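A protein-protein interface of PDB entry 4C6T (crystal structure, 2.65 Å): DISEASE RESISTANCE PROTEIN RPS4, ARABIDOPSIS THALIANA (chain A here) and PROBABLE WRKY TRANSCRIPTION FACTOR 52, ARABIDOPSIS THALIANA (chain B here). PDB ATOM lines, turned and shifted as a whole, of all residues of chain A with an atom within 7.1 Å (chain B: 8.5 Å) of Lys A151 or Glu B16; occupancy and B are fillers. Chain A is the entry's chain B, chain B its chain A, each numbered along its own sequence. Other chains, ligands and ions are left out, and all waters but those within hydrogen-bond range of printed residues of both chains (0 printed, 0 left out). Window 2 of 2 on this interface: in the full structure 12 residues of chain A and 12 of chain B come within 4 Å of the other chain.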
ATOM      1  N   TYR A 103      32.245 -17.287 -12.801  1.00  0.00           N
ATOM      2  CA  TYR A 103      31.792 -18.576 -13.281  1.00  0.00           C
ATOM      3  C   TYR A 103      32.313 -19.722 -12.439  1.00  0.00           C
ATOM      4  O   TYR A 103      33.426 -20.202 -12.630  1.00  0.00           O
ATOM      5  CB  TYR A 103      32.195 -18.786 -14.735  1.00  0.00           C
ATOM      6  CG  TYR A 103      31.553 -20.015 -15.298  1.00  0.00           C
ATOM      7  CD1 TYR A 103      30.236 -19.989 -15.727  1.00  0.00           C
ATOM      8  CD2 TYR A 103      32.247 -21.196 -15.402  1.00  0.00           C
ATOM      9  CE1 TYR A 103      29.624 -21.118 -16.230  1.00  0.00           C
ATOM     10  CE2 TYR A 103      31.640 -22.328 -15.919  1.00  0.00           C
ATOM     11  CZ  TYR A 103      30.329 -22.284 -16.324  1.00  0.00           C
ATOM     12  OH  TYR A 103      29.731 -23.410 -16.840  1.00  0.00           O
ATOM     13  N   LYS A 104      31.467 -20.159 -11.518  1.00  0.00           N
ATOM     14  CA  LYS A 104      31.693 -21.345 -10.689  1.00  0.00           C
ATOM     15  C   LYS A 104      32.902 -21.210  -9.763  1.00  0.00           C
ATOM     16  O   LYS A 104      33.512 -22.206  -9.364  1.00  0.00           O
ATOM     17  CB  LYS A 104      31.800 -22.607 -11.576  1.00  0.00           C
ATOM     18  CG  LYS A 104      30.430 -23.114 -12.079  1.00  0.00           C
ATOM     19  CD  LYS A 104      30.559 -24.225 -13.101  1.00  0.00           C
ATOM     20  CE  LYS A 104      29.209 -24.915 -13.376  1.00  0.00           C
ATOM     21  NZ  LYS A 104      28.205 -24.043 -14.047  1.00  0.00           N
ATOM     22  N   ILE A 149      27.702 -17.003 -10.781  1.00  0.00           N
ATOM     23  CA  ILE A 149      27.165 -18.260 -11.298  1.00  0.00           C
ATOM     24  C   ILE A 149      27.744 -19.450 -10.518  1.00  0.00           C
ATOM     25  O   ILE A 149      28.889 -19.837 -10.734  1.00  0.00           O
ATOM     26  CB  ILE A 149      27.478 -18.439 -12.812  1.00  0.00           C
ATOM     27  CG1 ILE A 149      26.934 -17.266 -13.628  1.00  0.00           C
ATOM     28  CG2 ILE A 149      26.890 -19.741 -13.342  1.00  0.00           C
ATOM     29  CD1 ILE A 149      27.478 -17.229 -15.043  1.00  0.00           C
ATOM     30  N   ASP A 150      26.964 -20.039  -9.620  1.00  0.00           N
ATOM     31  CA  ASP A 150      27.435 -21.221  -8.908  1.00  0.00           C
ATOM     32  C   ASP A 150      26.768 -22.459  -9.463  1.00  0.00           C
ATOM     33  O   ASP A 150      26.089 -22.382 -10.487  1.00  0.00           O
ATOM     34  CB  ASP A 150      27.192 -21.104  -7.412  1.00  0.00           C
ATOM     35  CG  ASP A 150      25.738 -20.960  -7.076  1.00  0.00           C
ATOM     36  OD1 ASP A 150      25.017 -21.989  -7.058  1.00  0.00           O
ATOM     37  OD2 ASP A 150      25.323 -19.814  -6.796  1.00  0.00           O
ATOM     38  N   LYS A 151      26.974 -23.606  -8.826  1.00  0.00           N
ATOM     39  CA  LYS A 151      26.542 -24.850  -9.452  1.00  0.00           C
ATOM     40  C   LYS A 151      25.039 -25.101  -9.297  1.00  0.00           C
ATOM     41  O   LYS A 151      24.477 -25.956  -9.983  1.00  0.00           O
ATOM     42  CB  LYS A 151      27.344 -26.034  -8.921  1.00  0.00           C
ATOM     43  CG  LYS A 151      27.242 -27.279  -9.828  1.00  0.00           C
ATOM     44  CD  LYS A 151      27.150 -26.912 -11.326  1.00  0.00           C
ATOM     45  CE  LYS A 151      26.733 -28.116 -12.182  1.00  0.00           C
ATOM     46  NZ  LYS A 151      26.767 -27.835 -13.655  1.00  0.00           N
ATOM     47  N   LYS A 152      24.390 -24.339  -8.421  1.00  0.00           N
ATOM     48  CA  LYS A 152      22.935 -24.401  -8.295  1.00  0.00           C
ATOM     49  C   LYS A 152      22.273 -23.300  -9.131  1.00  0.00           C
ATOM     50  O   LYS A 152      21.047 -23.147  -9.117  1.00  0.00           O
ATOM     51  CB  LYS A 152      22.498 -24.250  -6.829  1.00  0.00           C
ATOM     52  CG  LYS A 152      22.417 -25.542  -6.003  1.00  0.00           C
ATOM     53  CD  LYS A 152      21.923 -25.223  -4.577  1.00  0.00           C
ATOM     54  CE  LYS A 152      21.632 -26.478  -3.754  1.00  0.00           C
ATOM     55  NZ  LYS A 152      20.766 -27.455  -4.475  1.00  0.00           N
ATOM     56  N   SER A 153      23.076 -22.532  -9.857  1.00  0.00           N
ATOM     57  CA  SER A 153      22.521 -21.453 -10.653  1.00  0.00           C
ATOM     58  C   SER A 153      21.925 -21.989 -11.936  1.00  0.00           C
ATOM     59  O   SER A 153      22.495 -22.884 -12.578  1.00  0.00           O
ATOM     60  CB  SER A 153      23.591 -20.408 -10.976  1.00  0.00           C
ATOM     61  OG  SER A 153      23.866 -19.604  -9.843  1.00  0.00           O
ATOM     62  N   VAL A 154      20.792 -21.426 -12.331  1.00  0.00           N
ATOM     63  CA  VAL A 154      20.205 -21.781 -13.611  1.00  0.00           C
ATOM     64  C   VAL A 154      20.883 -20.973 -14.699  1.00  0.00           C
ATOM     65  O   VAL A 154      20.682 -19.770 -14.786  1.00  0.00           O
ATOM     66  CB  VAL A 154      18.687 -21.555 -13.622  1.00  0.00           C
ATOM     67  CG1 VAL A 154      18.095 -21.970 -14.963  1.00  0.00           C
ATOM     68  CG2 VAL A 154      18.080 -22.338 -12.519  1.00  0.00           C
ATOM     69  N   GLU A 155      21.704 -21.620 -15.513  1.00  0.00           N
ATOM     70  CA  GLU A 155      22.573 -20.856 -16.409  1.00  0.00           C
ATOM     71  C   GLU A 155      21.788 -20.001 -17.379  1.00  0.00           C
ATOM     72  O   GLU A 155      22.164 -18.870 -17.661  1.00  0.00           O
ATOM     73  CB  GLU A 155      23.514 -21.787 -17.175  1.00  0.00           C
ATOM     74  CG  GLU A 155      24.787 -22.076 -16.410  1.00  0.00           C
ATOM     75  CD  GLU A 155      25.785 -22.921 -17.180  1.00  0.00           C
ATOM     76  OE1 GLU A 155      25.591 -23.202 -18.398  1.00  0.00           O
ATOM     77  OE2 GLU A 155      26.792 -23.298 -16.552  1.00  0.00           O
ATOM     78  N   CYS B  13      16.618 -35.638 -17.771  1.00  0.00           N
ATOM     79  CA  CYS B  13      18.075 -35.596 -17.649  1.00  0.00           C
ATOM     80  C   CYS B  13      18.541 -35.913 -16.234  1.00  0.00           C
ATOM     81  O   CYS B  13      17.723 -36.017 -15.325  1.00  0.00           O
ATOM     82  CB  CYS B  13      18.599 -34.231 -18.059  1.00  0.00           C
ATOM     83  SG  CYS B  13      18.095 -33.029 -16.848  1.00  0.00           S
ATOM     84  N   VAL B  14      19.851 -36.078 -16.046  1.00  0.00           N
ATOM     85  CA  VAL B  14      20.382 -36.237 -14.688  1.00  0.00           C
ATOM     86  C   VAL B  14      20.657 -34.846 -14.100  1.00  0.00           C
ATOM     87  O   VAL B  14      20.600 -33.860 -14.828  1.00  0.00           O
ATOM     88  CB  VAL B  14      21.650 -37.080 -14.677  1.00  0.00           C
ATOM     89  CG1 VAL B  14      21.357 -38.460 -15.309  1.00  0.00           C
ATOM     90  CG2 VAL B  14      22.764 -36.363 -15.427  1.00  0.00           C
ATOM     91  N   GLU B  15      20.938 -34.766 -12.801  1.00  0.00           N
ATOM     92  CA  GLU B  15      21.078 -33.469 -12.119  1.00  0.00           C
ATOM     93  C   GLU B  15      22.268 -32.625 -12.587  1.00  0.00           C
ATOM     94  O   GLU B  15      22.160 -31.401 -12.693  1.00  0.00           O
ATOM     95  CB  GLU B  15      21.163 -33.675 -10.597  1.00  0.00           C
ATOM     96  CG  GLU B  15      19.812 -33.519  -9.904  1.00  0.00           C
ATOM     97  CD  GLU B  15      19.815 -34.008  -8.458  1.00  0.00           C
ATOM     98  OE1 GLU B  15      20.914 -34.066  -7.863  1.00  0.00           O
ATOM     99  OE2 GLU B  15      18.726 -34.358  -7.924  1.00  0.00           O
ATOM    100  N   GLU B  16      23.385 -33.272 -12.885  1.00  0.00           N
ATOM    101  CA  GLU B  16      24.606 -32.565 -13.267  1.00  0.00           C
ATOM    102  C   GLU B  16      24.395 -31.611 -14.451  1.00  0.00           C
ATOM    103  O   GLU B  16      25.017 -30.540 -14.502  1.00  0.00           O
ATOM    104  CB  GLU B  16      25.717 -33.580 -13.579  1.00  0.00           C
ATOM    105  CG  GLU B  16      26.165 -34.437 -12.366  1.00  0.00           C
ATOM    106  CD  GLU B  16      25.219 -35.617 -12.039  1.00  0.00           C
ATOM    107  OE1 GLU B  16      23.989 -35.506 -12.262  1.00  0.00           O
ATOM    108  OE2 GLU B  16      25.709 -36.656 -11.533  1.00  0.00           O
ATOM    109  N   VAL B  17      23.453 -31.932 -15.341  1.00  0.00           N
ATOM    110  CA  VAL B  17      23.212 -31.074 -16.505  1.00  0.00           C
ATOM    111  C   VAL B  17      21.943 -30.237 -16.372  1.00  0.00           C
ATOM    112  O   VAL B  17      21.650 -29.415 -17.235  1.00  0.00           O
ATOM    113  CB  VAL B  17      23.078 -31.872 -17.809  1.00  0.00           C
ATOM    114  CG1 VAL B  17      24.373 -32.581 -18.113  1.00  0.00           C
ATOM    115  CG2 VAL B  17      21.899 -32.826 -17.713  1.00  0.00           C
ATOM    116  N   ARG B  18      21.185 -30.468 -15.309  1.00  0.00           N
ATOM    117  CA  ARG B  18      19.905 -29.810 -15.141  1.00  0.00           C
ATOM    118  C   ARG B  18      20.042 -28.282 -15.195  1.00  0.00           C
ATOM    119  O   ARG B  18      19.324 -27.609 -15.933  1.00  0.00           O
ATOM    120  CB  ARG B  18      19.298 -30.230 -13.814  1.00  0.00           C
ATOM    121  CG  ARG B  18      17.919 -29.720 -13.559  1.00  0.00           C
ATOM    122  CD  ARG B  18      17.409 -30.367 -12.306  1.00  0.00           C
ATOM    123  NE  ARG B  18      15.999 -30.084 -12.098  1.00  0.00           N
ATOM    124  CZ  ARG B  18      15.344 -30.362 -10.980  1.00  0.00           C
ATOM    125  NH1 ARG B  18      15.980 -30.938  -9.961  1.00  0.00           N
ATOM    126  NH2 ARG B  18      14.054 -30.069 -10.890  1.00  0.00           N
ATOM    127  N   TYR B  19      21.011 -27.742 -14.464  1.00  0.00           N
ATOM    128  CA  TYR B  19      21.110 -26.302 -14.344  1.00  0.00           C
ATOM    129  C   TYR B  19      22.015 -25.704 -15.405  1.00  0.00           C
ATOM    130  O   TYR B  19      22.093 -24.488 -15.521  1.00  0.00           O
ATOM    131  CB  TYR B  19      21.608 -25.925 -12.954  1.00  0.00           C
ATOM    132  CG  TYR B  19      20.724 -26.479 -11.865  1.00  0.00           C
ATOM    133  CD1 TYR B  19      19.413 -26.040 -11.722  1.00  0.00           C
ATOM    134  CD2 TYR B  19      21.193 -27.461 -10.998  1.00  0.00           C
ATOM    135  CE1 TYR B  19      18.596 -26.558 -10.746  1.00  0.00           C
ATOM    136  CE2 TYR B  19      20.388 -27.987 -10.015  1.00  0.00           C
ATOM    137  CZ  TYR B  19      19.085 -27.534  -9.888  1.00  0.00           C
ATOM    138  OH  TYR B  19      18.263 -28.052  -8.902  1.00  0.00           O
ATOM    139  N   SER B  20      22.686 -26.534 -16.197  1.00  0.00           N
ATOM    140  CA  SER B  20      23.530 -25.982 -17.255  1.00  0.00           C
ATOM    141  C   SER B  20      22.903 -26.260 -18.616  1.00  0.00           C
ATOM    142  O   SER B  20      21.988 -25.536 -19.037  1.00  0.00           O
ATOM    143  CB  SER B  20      24.957 -26.540 -17.219  1.00  0.00           C
ATOM    144  OG  SER B  20      24.979 -27.951 -17.135  1.00  0.00           O
ATOM    145  N   PHE B  21      23.376 -27.311 -19.293  1.00  0.00           N
ATOM    146  CA  PHE B  21      22.961 -27.561 -20.678  1.00  0.00           C
ATOM    147  C   PHE B  21      21.439 -27.614 -20.852  1.00  0.00           C
ATOM    148  O   PHE B  21      20.905 -26.985 -21.761  1.00  0.00           O
ATOM    149  CB  PHE B  21      23.582 -28.862 -21.207  1.00  0.00           C
ATOM    150  CG  PHE B  21      23.108 -29.244 -22.586  1.00  0.00           C
ATOM    151  CD1 PHE B  21      23.512 -28.518 -23.701  1.00  0.00           C
ATOM    152  CD2 PHE B  21      22.284 -30.349 -22.774  1.00  0.00           C
ATOM    153  CE1 PHE B  21      23.096 -28.874 -24.973  1.00  0.00           C
ATOM    154  CE2 PHE B  21      21.858 -30.717 -24.050  1.00  0.00           C
ATOM    155  CZ  PHE B  21      22.254 -29.970 -25.146  1.00  0.00           C
ATOM    156  N   VAL B  22      20.743 -28.336 -19.978  1.00  0.00           N
ATOM    157  CA  VAL B  22      19.302 -28.488 -20.145  1.00  0.00           C
ATOM    158  C   VAL B  22      18.570 -27.157 -19.963  1.00  0.00           C
ATOM    159  O   VAL B  22      17.564 -26.921 -20.638  1.00  0.00           O
ATOM    160  CB  VAL B  22      18.711 -29.546 -19.177  1.00  0.00           C
ATOM    161  CG1 VAL B  22      17.199 -29.506 -19.167  1.00  0.00           C
ATOM    162  CG2 VAL B  22      19.176 -30.942 -19.568  1.00  0.00           C
ATOM    163  N   ASP B  40      13.834 -34.505 -13.563  1.00  0.00           N
ATOM    164  CA  ASP B  40      15.070 -35.038 -13.044  1.00  0.00           C
ATOM    165  C   ASP B  40      14.942 -36.523 -12.760  1.00  0.00           C
ATOM    166  O   ASP B  40      14.077 -36.942 -11.982  1.00  0.00           O
ATOM    167  CB  ASP B  40      15.438 -34.301 -11.764  1.00  0.00           C
ATOM    168  CG  ASP B  40      16.743 -34.766 -11.190  1.00  0.00           C
ATOM    169  OD1 ASP B  40      17.725 -34.864 -11.959  1.00  0.00           O
ATOM    170  OD2 ASP B  40      16.771 -35.055  -9.970  1.00  0.00           O
ATOM    171  N   VAL B  41      15.809 -37.325 -13.366  1.00  0.00           N
ATOM    172  CA  VAL B  41      15.678 -38.768 -13.236  1.00  0.00           C
ATOM    173  C   VAL B  41      16.482 -39.348 -12.073  1.00  0.00           C
ATOM    174  O   VAL B  41      16.419 -40.543 -11.820  1.00  0.00           O
ATOM    175  CB  VAL B  41      16.088 -39.480 -14.537  1.00  0.00           C
ATOM    176  CG1 VAL B  41      15.265 -38.963 -15.676  1.00  0.00           C
ATOM    177  CG2 VAL B  41      17.544 -39.258 -14.817  1.00  0.00           C
ATOM    178  N   ASP B  42      17.218 -38.504 -11.360  1.00  0.00           N
ATOM    179  CA  ASP B  42      18.021 -38.952 -10.225  1.00  0.00           C
ATOM    180  C   ASP B  42      17.138 -39.230  -9.014  1.00  0.00           C
ATOM    181  O   ASP B  42      17.609 -39.692  -7.967  1.00  0.00           O
ATOM    182  CB  ASP B  42      19.090 -37.917  -9.885  1.00  0.00           C
ATOM    183  CG  ASP B  42      20.259 -37.961 -10.845  1.00  0.00           C
ATOM    184  OD1 ASP B  42      20.340 -38.924 -11.626  1.00  0.00           O
ATOM    185  OD2 ASP B  42      21.080 -37.023 -10.849  1.00  0.00           O
ATOM    186  N   PRO B  66      23.555 -38.964 -19.996  1.00  0.00           N
ATOM    187  CA  PRO B  66      24.924 -38.664 -19.551  1.00  0.00           C
ATOM    188  C   PRO B  66      25.912 -39.499 -20.343  1.00  0.00           C
ATOM    189  O   PRO B  66      26.243 -40.619 -19.932  1.00  0.00           O
ATOM    190  CB  PRO B  66      24.922 -39.054 -18.063  1.00  0.00           C
ATOM    191  CG  PRO B  66      23.726 -39.973 -17.881  1.00  0.00           C
ATOM    192  CD  PRO B  66      22.938 -40.031 -19.191  1.00  0.00           C
ATOM    193  N   CYS B  69      29.172 -41.461 -19.221  1.00  0.00           N
ATOM    194  CA  CYS B  69      29.026 -42.594 -18.316  1.00  0.00           C
ATOM    195  C   CYS B  69      28.742 -43.897 -19.032  1.00  0.00           C
ATOM    196  O   CYS B  69      28.251 -43.894 -20.150  1.00  0.00           O
ATOM    197  CB  CYS B  69      27.893 -42.336 -17.324  1.00  0.00           C
ATOM    198  SG  CYS B  69      28.062 -40.882 -16.280  1.00  0.00           S
ATOM    199  N   LYS B  78      17.935 -45.302 -14.449  1.00  0.00           N
ATOM    200  CA  LYS B  78      17.411 -43.932 -14.568  1.00  0.00           C
ATOM    201  C   LYS B  78      16.442 -43.657 -15.728  1.00  0.00           C
ATOM    202  O   LYS B  78      15.463 -42.922 -15.553  1.00  0.00           O
ATOM    203  CB  LYS B  78      18.575 -42.939 -14.671  1.00  0.00           C
ATOM    204  CG  LYS B  78      19.469 -42.900 -13.448  1.00  0.00           C
ATOM    205  CD  LYS B  78      20.580 -41.884 -13.656  1.00  0.00           C
ATOM    206  CE  LYS B  78      21.475 -41.756 -12.427  1.00  0.00           C
ATOM    207  NZ  LYS B  78      22.618 -40.823 -12.681  1.00  0.00           N
ATOM    208  N   TYR B  99      24.894 -36.263 -24.464  1.00  0.00           N
ATOM    209  CA  TYR B  99      25.581 -35.037 -24.097  1.00  0.00           C
ATOM    210  C   TYR B  99      26.859 -35.330 -23.299  1.00  0.00           C
ATOM    211  O   TYR B  99      26.849 -36.151 -22.386  1.00  0.00           O
ATOM    212  CB  TYR B  99      24.642 -34.135 -23.293  1.00  0.00           C
ATOM    213  CG  TYR B  99      25.303 -32.842 -22.952  1.00  0.00           C
ATOM    214  CD1 TYR B  99      25.369 -31.792 -23.873  1.00  0.00           C
ATOM    215  CD2 TYR B  99      25.955 -32.692 -21.732  1.00  0.00           C
ATOM    216  CE1 TYR B  99      26.026 -30.603 -23.549  1.00  0.00           C
ATOM    217  CE2 TYR B  99      26.620 -31.526 -21.418  1.00  0.00           C
ATOM    218  CZ  TYR B  99      26.647 -30.484 -22.319  1.00  0.00           C
ATOM    219  OH  TYR B  99      27.292 -29.343 -21.963  1.00  0.00           O
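NZ of Lys A151 lies within hydrogen-bond range of O of Glu B16 (3.3 Å). O of Tyr B19 sits at hydrogen-bond distance from N of Glu A155, at 2.9 Å. The backbone carbonyl oxygen of Tyr B19 sits close to the backbone carbonyl oxygen of Ser A153, 3.4 Å away.
The backbone NH (N) of Asp A150 lies within hydrogen-bond range of the side-chain hydroxyl (OG) of Ser A153 (3.1 Å). The side-chain amino group (NZ) of Lys A104 lies within salt-bridge range of the side-chain carboxylate (OE2) of Glu A155. The side-chain carboxylate of Glu A155 is in hydrogen-bond range of the side-chain hydroxyl of Tyr A103.
Among the printed residues, pairs that only touch across the chains: Lys A151 with Tyr B19, Lys A151 with Ser B20, Val A154 with Tyr B19 and Glu A155 with Ser B20.
Of chain B, only Glu B16 (3.3 Å), Tyr B19 (3.8 Å) and Ser B20 (3.9 Å) come within 4 Å of Lys A151. Glu B16 touches just one residue of chain A: Lys A151. Of the printed residues of chain B, Glu A155 touches Tyr B19 (2.9 Å) and Ser B20 (3.6 Å). Of the printed residues of chain A, Tyr B19 touches Lys A151, Ser A153, Val A154 and Glu A155. Val B14 touches none of the printed residues of chain A. The nearest residue of chain B that does not touch Lys A151 is Val B17 (5.5 Å). The nearest printed residue of chain A that does not touch Tyr B19 is Lys A152 (4.2 Å).
Of the 9 printed residues of chain A, 4 touch a printed residue of chain B. Printed residues of chain B that touch a printed residue of chain A: Glu B16, Tyr B19 and Ser B20. Among the printed residues, 7 pairs touch across the chains.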
